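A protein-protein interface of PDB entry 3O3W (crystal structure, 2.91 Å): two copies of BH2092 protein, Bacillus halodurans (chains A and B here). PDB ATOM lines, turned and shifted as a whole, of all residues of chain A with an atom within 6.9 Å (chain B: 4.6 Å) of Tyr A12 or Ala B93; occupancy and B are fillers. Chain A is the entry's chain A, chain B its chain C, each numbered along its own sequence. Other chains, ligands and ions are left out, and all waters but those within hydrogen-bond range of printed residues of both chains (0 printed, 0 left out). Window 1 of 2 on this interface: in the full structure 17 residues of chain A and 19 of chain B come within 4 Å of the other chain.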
ATOM      1  N   ALA A   3      20.762 -17.969  19.623  1.00  0.00           N
ATOM      2  CA  ALA A   3      22.166 -17.711  19.388  1.00  0.00           C
ATOM      3  C   ALA A   3      23.138 -18.783  19.852  1.00  0.00           C
ATOM      4  O   ALA A   3      22.836 -19.564  20.755  1.00  0.00           O
ATOM      5  CB  ALA A   3      22.513 -16.397  20.001  1.00  0.00           C
ATOM      6  N   PRO A   5      26.166 -20.950  21.533  1.00  0.00           N
ATOM      7  CA  PRO A   5      26.582 -20.917  22.931  1.00  0.00           C
ATOM      8  C   PRO A   5      27.562 -19.833  23.352  1.00  0.00           C
ATOM      9  O   PRO A   5      27.276 -19.081  24.274  1.00  0.00           O
ATOM     10  CB  PRO A   5      27.114 -22.329  23.168  1.00  0.00           C
ATOM     11  CG  PRO A   5      26.280 -23.157  22.224  1.00  0.00           C
ATOM     12  CD  PRO A   5      26.307 -22.310  20.972  1.00  0.00           C
ATOM     13  N   GLU A   7      28.619 -17.060  21.713  1.00  0.00           N
ATOM     14  CA  GLU A   7      28.119 -15.727  21.407  1.00  0.00           C
ATOM     15  C   GLU A   7      27.127 -15.306  22.484  1.00  0.00           C
ATOM     16  O   GLU A   7      27.177 -14.178  22.984  1.00  0.00           O
ATOM     17  CB  GLU A   7      27.437 -15.723  20.037  1.00  0.00           C
ATOM     18  CG  GLU A   7      27.057 -14.331  19.543  1.00  0.00           C
ATOM     19  CD  GLU A   7      26.389 -14.352  18.177  1.00  0.00           C
ATOM     20  OE1 GLU A   7      26.938 -14.995  17.249  1.00  0.00           O
ATOM     21  OE2 GLU A   7      25.320 -13.713  18.023  1.00  0.00           O
ATOM     22  N   ALA A   8      26.233 -16.225  22.841  1.00  0.00           N
ATOM     23  CA  ALA A   8      25.224 -15.971  23.861  1.00  0.00           C
ATOM     24  C   ALA A   8      25.876 -15.669  25.208  1.00  0.00           C
ATOM     25  O   ALA A   8      25.530 -14.683  25.866  1.00  0.00           O
ATOM     26  CB  ALA A   8      24.299 -17.168  23.985  1.00  0.00           C
ATOM     27  N   TYR A   9      26.825 -16.508  25.614  1.00  0.00           N
ATOM     28  CA  TYR A   9      27.500 -16.306  26.884  1.00  0.00           C
ATOM     29  C   TYR A   9      28.066 -14.891  26.985  1.00  0.00           C
ATOM     30  O   TYR A   9      27.839 -14.216  27.987  1.00  0.00           O
ATOM     31  CB  TYR A   9      28.620 -17.326  27.069  1.00  0.00           C
ATOM     32  CG  TYR A   9      29.289 -17.234  28.428  1.00  0.00           C
ATOM     33  CD1 TYR A   9      28.559 -17.433  29.598  1.00  0.00           C
ATOM     34  CD2 TYR A   9      30.647 -16.924  28.548  1.00  0.00           C
ATOM     35  CE1 TYR A   9      29.164 -17.326  30.860  1.00  0.00           C
ATOM     36  CE2 TYR A   9      31.261 -16.811  29.798  1.00  0.00           C
ATOM     37  CZ  TYR A   9      30.520 -17.010  30.944  1.00  0.00           C
ATOM     38  OH  TYR A   9      31.131 -16.882  32.170  1.00  0.00           O
ATOM     39  N   ARG A  10      28.786 -14.440  25.959  1.00  0.00           N
ATOM     40  CA  ARG A  10      29.355 -13.101  25.982  1.00  0.00           C
ATOM     41  C   ARG A  10      28.287 -12.044  26.040  1.00  0.00           C
ATOM     42  O   ARG A  10      28.453 -11.017  26.703  1.00  0.00           O
ATOM     43  CB  ARG A  10      30.220 -12.854  24.754  1.00  0.00           C
ATOM     44  CG  ARG A  10      31.536 -13.577  24.804  1.00  0.00           C
ATOM     45  CD  ARG A  10      32.347 -13.338  23.547  1.00  0.00           C
ATOM     46  NE  ARG A  10      33.179 -14.496  23.270  1.00  0.00           N
ATOM     47  CZ  ARG A  10      32.823 -15.566  22.569  1.00  0.00           C
ATOM     48  NH1 ARG A  10      31.621 -15.669  22.017  1.00  0.00           N
ATOM     49  NH2 ARG A  10      33.693 -16.557  22.460  1.00  0.00           N
ATOM     50  N   HIS A  11      27.190 -12.286  25.341  1.00  0.00           N
ATOM     51  CA  HIS A  11      26.096 -11.328  25.331  1.00  0.00           C
ATOM     52  C   HIS A  11      25.506 -11.136  26.734  1.00  0.00           C
ATOM     53  O   HIS A  11      25.413 -10.006  27.229  1.00  0.00           O
ATOM     54  CB  HIS A  11      25.002 -11.808  24.391  1.00  0.00           C
ATOM     55  CG  HIS A  11      23.773 -10.956  24.418  1.00  0.00           C
ATOM     56  ND1 HIS A  11      23.721  -9.709  23.835  1.00  0.00           N
ATOM     57  CD2 HIS A  11      22.563 -11.159  24.987  1.00  0.00           C
ATOM     58  CE1 HIS A  11      22.526  -9.178  24.044  1.00  0.00           C
ATOM     59  NE2 HIS A  11      21.805 -10.039  24.743  1.00  0.00           N
ATOM     60  N   TYR A  12      25.116 -12.244  27.368  1.00  0.00           N
ATOM     61  CA  TYR A  12      24.526 -12.207  28.705  1.00  0.00           C
ATOM     62  C   TYR A  12      25.501 -11.692  29.760  1.00  0.00           C
ATOM     63  O   TYR A  12      25.102 -11.024  30.712  1.00  0.00           O
ATOM     64  CB  TYR A  12      24.020 -13.597  29.094  1.00  0.00           C
ATOM     65  CG  TYR A  12      22.906 -14.111  28.202  1.00  0.00           C
ATOM     66  CD1 TYR A  12      21.701 -13.427  28.101  1.00  0.00           C
ATOM     67  CD2 TYR A  12      23.071 -15.271  27.434  1.00  0.00           C
ATOM     68  CE1 TYR A  12      20.692 -13.866  27.255  1.00  0.00           C
ATOM     69  CE2 TYR A  12      22.068 -15.726  26.590  1.00  0.00           C
ATOM     70  CZ  TYR A  12      20.875 -15.012  26.502  1.00  0.00           C
ATOM     71  OH  TYR A  12      19.879 -15.444  25.655  1.00  0.00           O
ATOM     72  N   MET A  13      26.777 -12.013  29.593  1.00  0.00           N
ATOM     73  CA  MET A  13      27.780 -11.556  30.525  1.00  0.00           C
ATOM     74  C   MET A  13      27.928 -10.042  30.424  1.00  0.00           C
ATOM     75  O   MET A  13      27.888  -9.339  31.433  1.00  0.00           O
ATOM     76  CB  MET A  13      29.118 -12.243  30.251  1.00  0.00           C
ATOM     77  CG  MET A  13      29.216 -13.687  30.769  1.00  0.00           C
ATOM     78  SD  MET A  13      28.786 -13.936  32.700  1.00  0.00           S
ATOM     79  CE  MET A  13      29.769 -12.424  33.460  1.00  0.00           C
ATOM     80  N   LYS A  14      28.089  -9.530  29.212  1.00  0.00           N
ATOM     81  CA  LYS A  14      28.225  -8.083  29.024  1.00  0.00           C
ATOM     82  C   LYS A  14      26.995  -7.337  29.538  1.00  0.00           C
ATOM     83  O   LYS A  14      27.105  -6.328  30.221  1.00  0.00           O
ATOM     84  CB  LYS A  14      28.453  -7.744  27.541  1.00  0.00           C
ATOM     85  CG  LYS A  14      29.832  -8.145  27.014  1.00  0.00           C
ATOM     86  CD  LYS A  14      30.046  -7.749  25.538  1.00  0.00           C
ATOM     87  CE  LYS A  14      29.963  -6.226  25.325  1.00  0.00           C
ATOM     88  NZ  LYS A  14      30.077  -5.791  23.895  1.00  0.00           N
ATOM     89  N   LYS A  15      25.821  -7.844  29.202  1.00  0.00           N
ATOM     90  CA  LYS A  15      24.582  -7.225  29.635  1.00  0.00           C
ATOM     91  C   LYS A  15      24.600  -7.058  31.154  1.00  0.00           C
ATOM     92  O   LYS A  15      24.287  -5.987  31.683  1.00  0.00           O
ATOM     93  CB  LYS A  15      23.407  -8.103  29.219  1.00  0.00           C
ATOM     94  CG  LYS A  15      22.063  -7.537  29.564  1.00  0.00           C
ATOM     95  CD  LYS A  15      20.976  -8.526  29.213  1.00  0.00           C
ATOM     96  CE  LYS A  15      19.607  -7.941  29.496  1.00  0.00           C
ATOM     97  NZ  LYS A  15      18.526  -8.893  29.140  1.00  0.00           N
ATOM     98  N   LEU A  16      24.977  -8.121  31.853  1.00  0.00           N
ATOM     99  CA  LEU A  16      25.037  -8.082  33.302  1.00  0.00           C
ATOM    100  C   LEU A  16      26.035  -7.065  33.826  1.00  0.00           C
ATOM    101  O   LEU A  16      25.904  -6.588  34.956  1.00  0.00           O
ATOM    102  CB  LEU A  16      25.399  -9.448  33.859  1.00  0.00           C
ATOM    103  CG  LEU A  16      24.321 -10.503  33.716  1.00  0.00           C
ATOM    104  CD1 LEU A  16      24.937 -11.844  34.043  1.00  0.00           C
ATOM    105  CD2 LEU A  16      23.124 -10.195  34.624  1.00  0.00           C
ATOM    106  N   SER A  17      27.039  -6.737  33.022  1.00  0.00           N
ATOM    107  CA  SER A  17      28.054  -5.773  33.449  1.00  0.00           C
ATOM    108  C   SER A  17      27.625  -4.320  33.224  1.00  0.00           C
ATOM    109  O   SER A  17      28.211  -3.388  33.774  1.00  0.00           O
ATOM    110  CB  SER A  17      29.360  -6.016  32.695  1.00  0.00           C
ATOM    111  OG  SER A  17      29.332  -5.432  31.402  1.00  0.00           O
ATOM    112  N   TYR B  18      18.439 -13.718  21.281  1.00  0.00           N
ATOM    113  CA  TYR B  18      18.841 -13.857  22.669  1.00  0.00           C
ATOM    114  C   TYR B  18      17.662 -13.910  23.639  1.00  0.00           C
ATOM    115  O   TYR B  18      17.740 -14.520  24.698  1.00  0.00           O
ATOM    116  CB  TYR B  18      19.772 -12.708  23.074  1.00  0.00           C
ATOM    117  CG  TYR B  18      21.101 -12.659  22.338  1.00  0.00           C
ATOM    118  CD1 TYR B  18      21.974 -13.748  22.354  1.00  0.00           C
ATOM    119  CD2 TYR B  18      21.513 -11.497  21.673  1.00  0.00           C
ATOM    120  CE1 TYR B  18      23.223 -13.681  21.735  1.00  0.00           C
ATOM    121  CE2 TYR B  18      22.761 -11.423  21.053  1.00  0.00           C
ATOM    122  CZ  TYR B  18      23.610 -12.520  21.093  1.00  0.00           C
ATOM    123  OH  TYR B  18      24.856 -12.432  20.504  1.00  0.00           O
ATOM    124  N   THR B  79      15.089 -19.999  30.101  1.00  0.00           N
ATOM    125  CA  THR B  79      15.047 -19.686  31.517  1.00  0.00           C
ATOM    126  C   THR B  79      14.070 -18.566  31.802  1.00  0.00           C
ATOM    127  O   THR B  79      13.722 -17.786  30.901  1.00  0.00           O
ATOM    128  CB  THR B  79      16.424 -19.252  32.031  1.00  0.00           C
ATOM    129  OG1 THR B  79      16.801 -18.014  31.412  1.00  0.00           O
ATOM    130  CG2 THR B  79      17.467 -20.317  31.717  1.00  0.00           C
ATOM    131  N   GLY B  88      17.697 -13.255  37.531  1.00  0.00           N
ATOM    132  CA  GLY B  88      17.729 -14.696  37.463  1.00  0.00           C
ATOM    133  C   GLY B  88      17.812 -15.260  36.072  1.00  0.00           C
ATOM    134  O   GLY B  88      18.739 -16.008  35.764  1.00  0.00           O
ATOM    135  N   ALA B  89      16.847 -14.906  35.230  1.00  0.00           N
ATOM    136  CA  ALA B  89      16.812 -15.409  33.860  1.00  0.00           C
ATOM    137  C   ALA B  89      18.102 -15.103  33.087  1.00  0.00           C
ATOM    138  O   ALA B  89      18.643 -15.994  32.420  1.00  0.00           O
ATOM    139  CB  ALA B  89      15.608 -14.846  33.128  1.00  0.00           C
ATOM    140  N   THR B  90      18.587 -13.865  33.178  1.00  0.00           N
ATOM    141  CA  THR B  90      19.811 -13.475  32.493  1.00  0.00           C
ATOM    142  C   THR B  90      21.034 -14.186  33.069  1.00  0.00           C
ATOM    143  O   THR B  90      21.856 -14.743  32.331  1.00  0.00           O
ATOM    144  CB  THR B  90      20.043 -11.963  32.589  1.00  0.00           C
ATOM    145  OG1 THR B  90      18.928 -11.262  32.022  1.00  0.00           O
ATOM    146  CG2 THR B  90      21.309 -11.568  31.829  1.00  0.00           C
ATOM    147  N   LYS B  91      21.155 -14.171  34.391  1.00  0.00           N
ATOM    148  CA  LYS B  91      22.274 -14.834  35.047  1.00  0.00           C
ATOM    149  C   LYS B  91      22.278 -16.303  34.652  1.00  0.00           C
ATOM    150  O   LYS B  91      23.285 -16.813  34.163  1.00  0.00           O
ATOM    151  CB  LYS B  91      22.154 -14.709  36.567  1.00  0.00           C
ATOM    152  CG  LYS B  91      22.421 -13.311  37.100  1.00  0.00           C
ATOM    153  CD  LYS B  91      22.338 -13.262  38.616  1.00  0.00           C
ATOM    154  CE  LYS B  91      22.572 -11.859  39.147  1.00  0.00           C
ATOM    155  NZ  LYS B  91      22.477 -11.796  40.642  1.00  0.00           N
ATOM    156  N   ALA B  92      21.140 -16.971  34.848  1.00  0.00           N
ATOM    157  CA  ALA B  92      21.001 -18.389  34.514  1.00  0.00           C
ATOM    158  C   ALA B  92      21.335 -18.640  33.043  1.00  0.00           C
ATOM    159  O   ALA B  92      22.013 -19.609  32.698  1.00  0.00           O
ATOM    160  CB  ALA B  92      19.588 -18.860  34.822  1.00  0.00           C
ATOM    161  N   ALA B  93      20.862 -17.759  32.175  1.00  0.00           N
ATOM    162  CA  ALA B  93      21.131 -17.909  30.760  1.00  0.00           C
ATOM    163  C   ALA B  93      22.631 -17.994  30.508  1.00  0.00           C
ATOM    164  O   ALA B  93      23.093 -18.752  29.659  1.00  0.00           O
ATOM    165  CB  ALA B  93      20.531 -16.741  29.988  1.00  0.00           C
ATOM    166  N   ALA B  94      23.393 -17.209  31.250  1.00  0.00           N
ATOM    167  CA  ALA B  94      24.842 -17.206  31.085  1.00  0.00           C
ATOM    168  C   ALA B  94      25.413 -18.556  31.460  1.00  0.00           C
ATOM    169  O   ALA B  94      26.237 -19.098  30.737  1.00  0.00           O
ATOM    170  CB  ALA B  94      25.479 -16.122  31.951  1.00  0.00           C
ATOM    171  N   LYS B  95      24.976 -19.102  32.590  1.00  0.00           N
ATOM    172  CA  LYS B  95      25.492 -20.390  33.037  1.00  0.00           C
ATOM    173  C   LYS B  95      25.189 -21.505  32.040  1.00  0.00           C
ATOM    174  O   LYS B  95      26.017 -22.391  31.815  1.00  0.00           O
ATOM    175  CB  LYS B  95      24.943 -20.713  34.431  1.00  0.00           C
ATOM    176  CG  LYS B  95      25.355 -19.674  35.452  1.00  0.00           C
ATOM    177  CD  LYS B  95      24.907 -20.008  36.860  1.00  0.00           C
ATOM    178  CE  LYS B  95      25.361 -18.915  37.838  1.00  0.00           C
ATOM    179  NZ  LYS B  95      25.012 -19.217  39.256  1.00  0.00           N
ATOM    180  N   PHE B  96      24.011 -21.449  31.428  1.00  0.00           N
ATOM    181  CA  PHE B  96      23.627 -22.456  30.443  1.00  0.00           C
ATOM    182  C   PHE B  96      24.459 -22.327  29.173  1.00  0.00           C
ATOM    183  O   PHE B  96      24.961 -23.316  28.646  1.00  0.00           O
ATOM    184  CB  PHE B  96      22.141 -22.335  30.114  1.00  0.00           C
ATOM    185  CG  PHE B  96      21.242 -23.058  31.079  1.00  0.00           C
ATOM    186  CD1 PHE B  96      21.227 -24.444  31.118  1.00  0.00           C
ATOM    187  CD2 PHE B  96      20.404 -22.361  31.944  1.00  0.00           C
ATOM    188  CE1 PHE B  96      20.389 -25.126  31.996  1.00  0.00           C
ATOM    189  CE2 PHE B  96      19.563 -23.041  32.824  1.00  0.00           C
ATOM    190  CZ  PHE B  96      19.560 -24.426  32.847  1.00  0.00           C
ATOM    191  N   ALA B  97      24.612 -21.098  28.691  1.00  0.00           N
ATOM    192  CA  ALA B  97      25.400 -20.843  27.498  1.00  0.00           C
ATOM    193  C   ALA B  97      26.828 -21.275  27.771  1.00  0.00           C
ATOM    194  O   ALA B  97      27.529 -21.737  26.877  1.00  0.00           O
ATOM    195  CB  ALA B  97      25.362 -19.371  27.148  1.00  0.00           C
ATOM    196  N   VAL B 103      20.793 -21.577  25.018  1.00  0.00           N
ATOM    197  CA  VAL B 103      19.896 -20.880  25.932  1.00  0.00           C
ATOM    198  C   VAL B 103      19.185 -19.658  25.357  1.00  0.00           C
ATOM    199  O   VAL B 103      19.634 -19.046  24.386  1.00  0.00           O
ATOM    200  CB  VAL B 103      20.665 -20.433  27.186  1.00  0.00           C
ATOM    201  CG1 VAL B 103      21.588 -19.279  26.831  1.00  0.00           C
ATOM    202  CG2 VAL B 103      19.698 -20.053  28.295  1.00  0.00           C
ATOM    203  N   LYS B 104      18.070 -19.302  25.984  1.00  0.00           N
ATOM    204  CA  LYS B 104      17.286 -18.139  25.583  1.00  0.00           C
ATOM    205  C   LYS B 104      16.482 -17.700  26.813  1.00  0.00           C
ATOM    206  O   LYS B 104      15.753 -18.504  27.383  1.00  0.00           O
ATOM    207  CB  LYS B 104      16.356 -18.533  24.442  1.00  0.00           C
ATOM    208  CG  LYS B 104      16.043 -17.417  23.477  1.00  0.00           C
ATOM    209  CD  LYS B 104      15.376 -17.975  22.243  1.00  0.00           C
ATOM    210  CE  LYS B 104      15.470 -17.004  21.094  1.00  0.00           C
ATOM    211  NZ  LYS B 104      14.945 -17.559  19.821  1.00  0.00           N
ATOM    212  N   GLU B 105      16.616 -16.444  27.229  1.00  0.00           N
ATOM    213  CA  GLU B 105      15.888 -15.988  28.405  1.00  0.00           C
ATOM    214  C   GLU B 105      14.480 -15.493  28.084  1.00  0.00           C
ATOM    215  O   GLU B 105      14.224 -14.965  27.001  1.00  0.00           O
ATOM    216  CB  GLU B 105      16.669 -14.893  29.138  1.00  0.00           C
ATOM    217  CG  GLU B 105      16.927 -13.658  28.299  1.00  0.00           C
ATOM    218  CD  GLU B 105      17.379 -12.465  29.121  1.00  0.00           C
ATOM    219  OE1 GLU B 105      16.704 -12.159  30.132  1.00  0.00           O
ATOM    220  OE2 GLU B 105      18.394 -11.826  28.749  1.00  0.00           O
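The backbone carbonyl oxygen (O) of Tyr B18 sits at hydrogen-bond distance from the backbone NH (N) of Glu B105.
The backbone NH (N) of Thr B79 is in hydrogen-bond range of the backbone carbonyl oxygen (O) of Lys B104 (3.2 Å).
The side-chain carboxylate of Glu B105 is in hydrogen-bond range of the side-chain hydroxyl of Thr B90, 3.1 Å away.
OH of Tyr B18 is in hydrogen-bond range of OE2 of Glu A7.
The side-chain hydroxyl (OH) of Tyr A12 is in hydrogen-bond range of the backbone carbonyl oxygen (O) of Tyr B18 (2.5 Å).
The side-chain amino group of Lys A15 is in salt-bridge range of the side-chain carboxylate of Glu B105, at 3.0 Å.
Among the printed residues, merely in contact across the chains: Tyr A9 with Ala B94 (3.1 Å), Ala A3 with Tyr B18 (3.3 Å), His A11 with Tyr B18 (3.4 Å), Tyr A12 with Glu B105 (3.4 Å), Pro A5 with Ala B97 (3.5 Å), Tyr A9 with Ala B97 (3.6 Å), Tyr A12 with Val B103 (3.6 Å), Leu A16 with Thr B90 (3.6 Å), Ala A8 with Tyr B18 (3.7 Å), Tyr A12 with Lys B104 (3.7 Å), Lys A15 with Thr B90 (3.8 Å), Tyr A12 with Ala B93 (3.9 Å), Tyr A12 with Thr B90 (3.99 Å) and Ala A8 with Ala B97 (3.998 Å).
Of the 13 printed residues of chain A, 9 touch a printed residue of chain B.
Of the 15 printed residues of chain B, 8 touch a printed residue of chain A.
Hydrophobic or aromatic side chains of chain B that line the printed part of chain A: Tyr B18, Ala B93, Ala B97 and Val B103.
Along chain B the printed residues that touch a printed residue of chain A span positions 18 to 105.
Among the printed residues, 17 pairs touch across the chains.
No position is printed for both chains.
Of the 17 pairs that touch across the chains among the printed residues, none has its exchanged pair printed and touching as well.
Printed residues of chain B within 4 Å of Tyr A12: Tyr B18 (2.5 Å), Thr B90 (3.99 Å), Ala B93 (3.9 Å), Val B103 (3.6 Å), Lys B104 (3.7 Å) and Glu B105 (3.4 Å).
Of the printed residues of chain A, Thr B90 touches Tyr A12, Lys A15 and Leu A16.
Ala B93 touches one residue of chain A.
Printed residues of chain A within 4 Å of Lys B104: Tyr A12 (3.7 Å).
The nearest residue of chain A that does not touch Ala B93 is Tyr A9 (5.6 Å).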
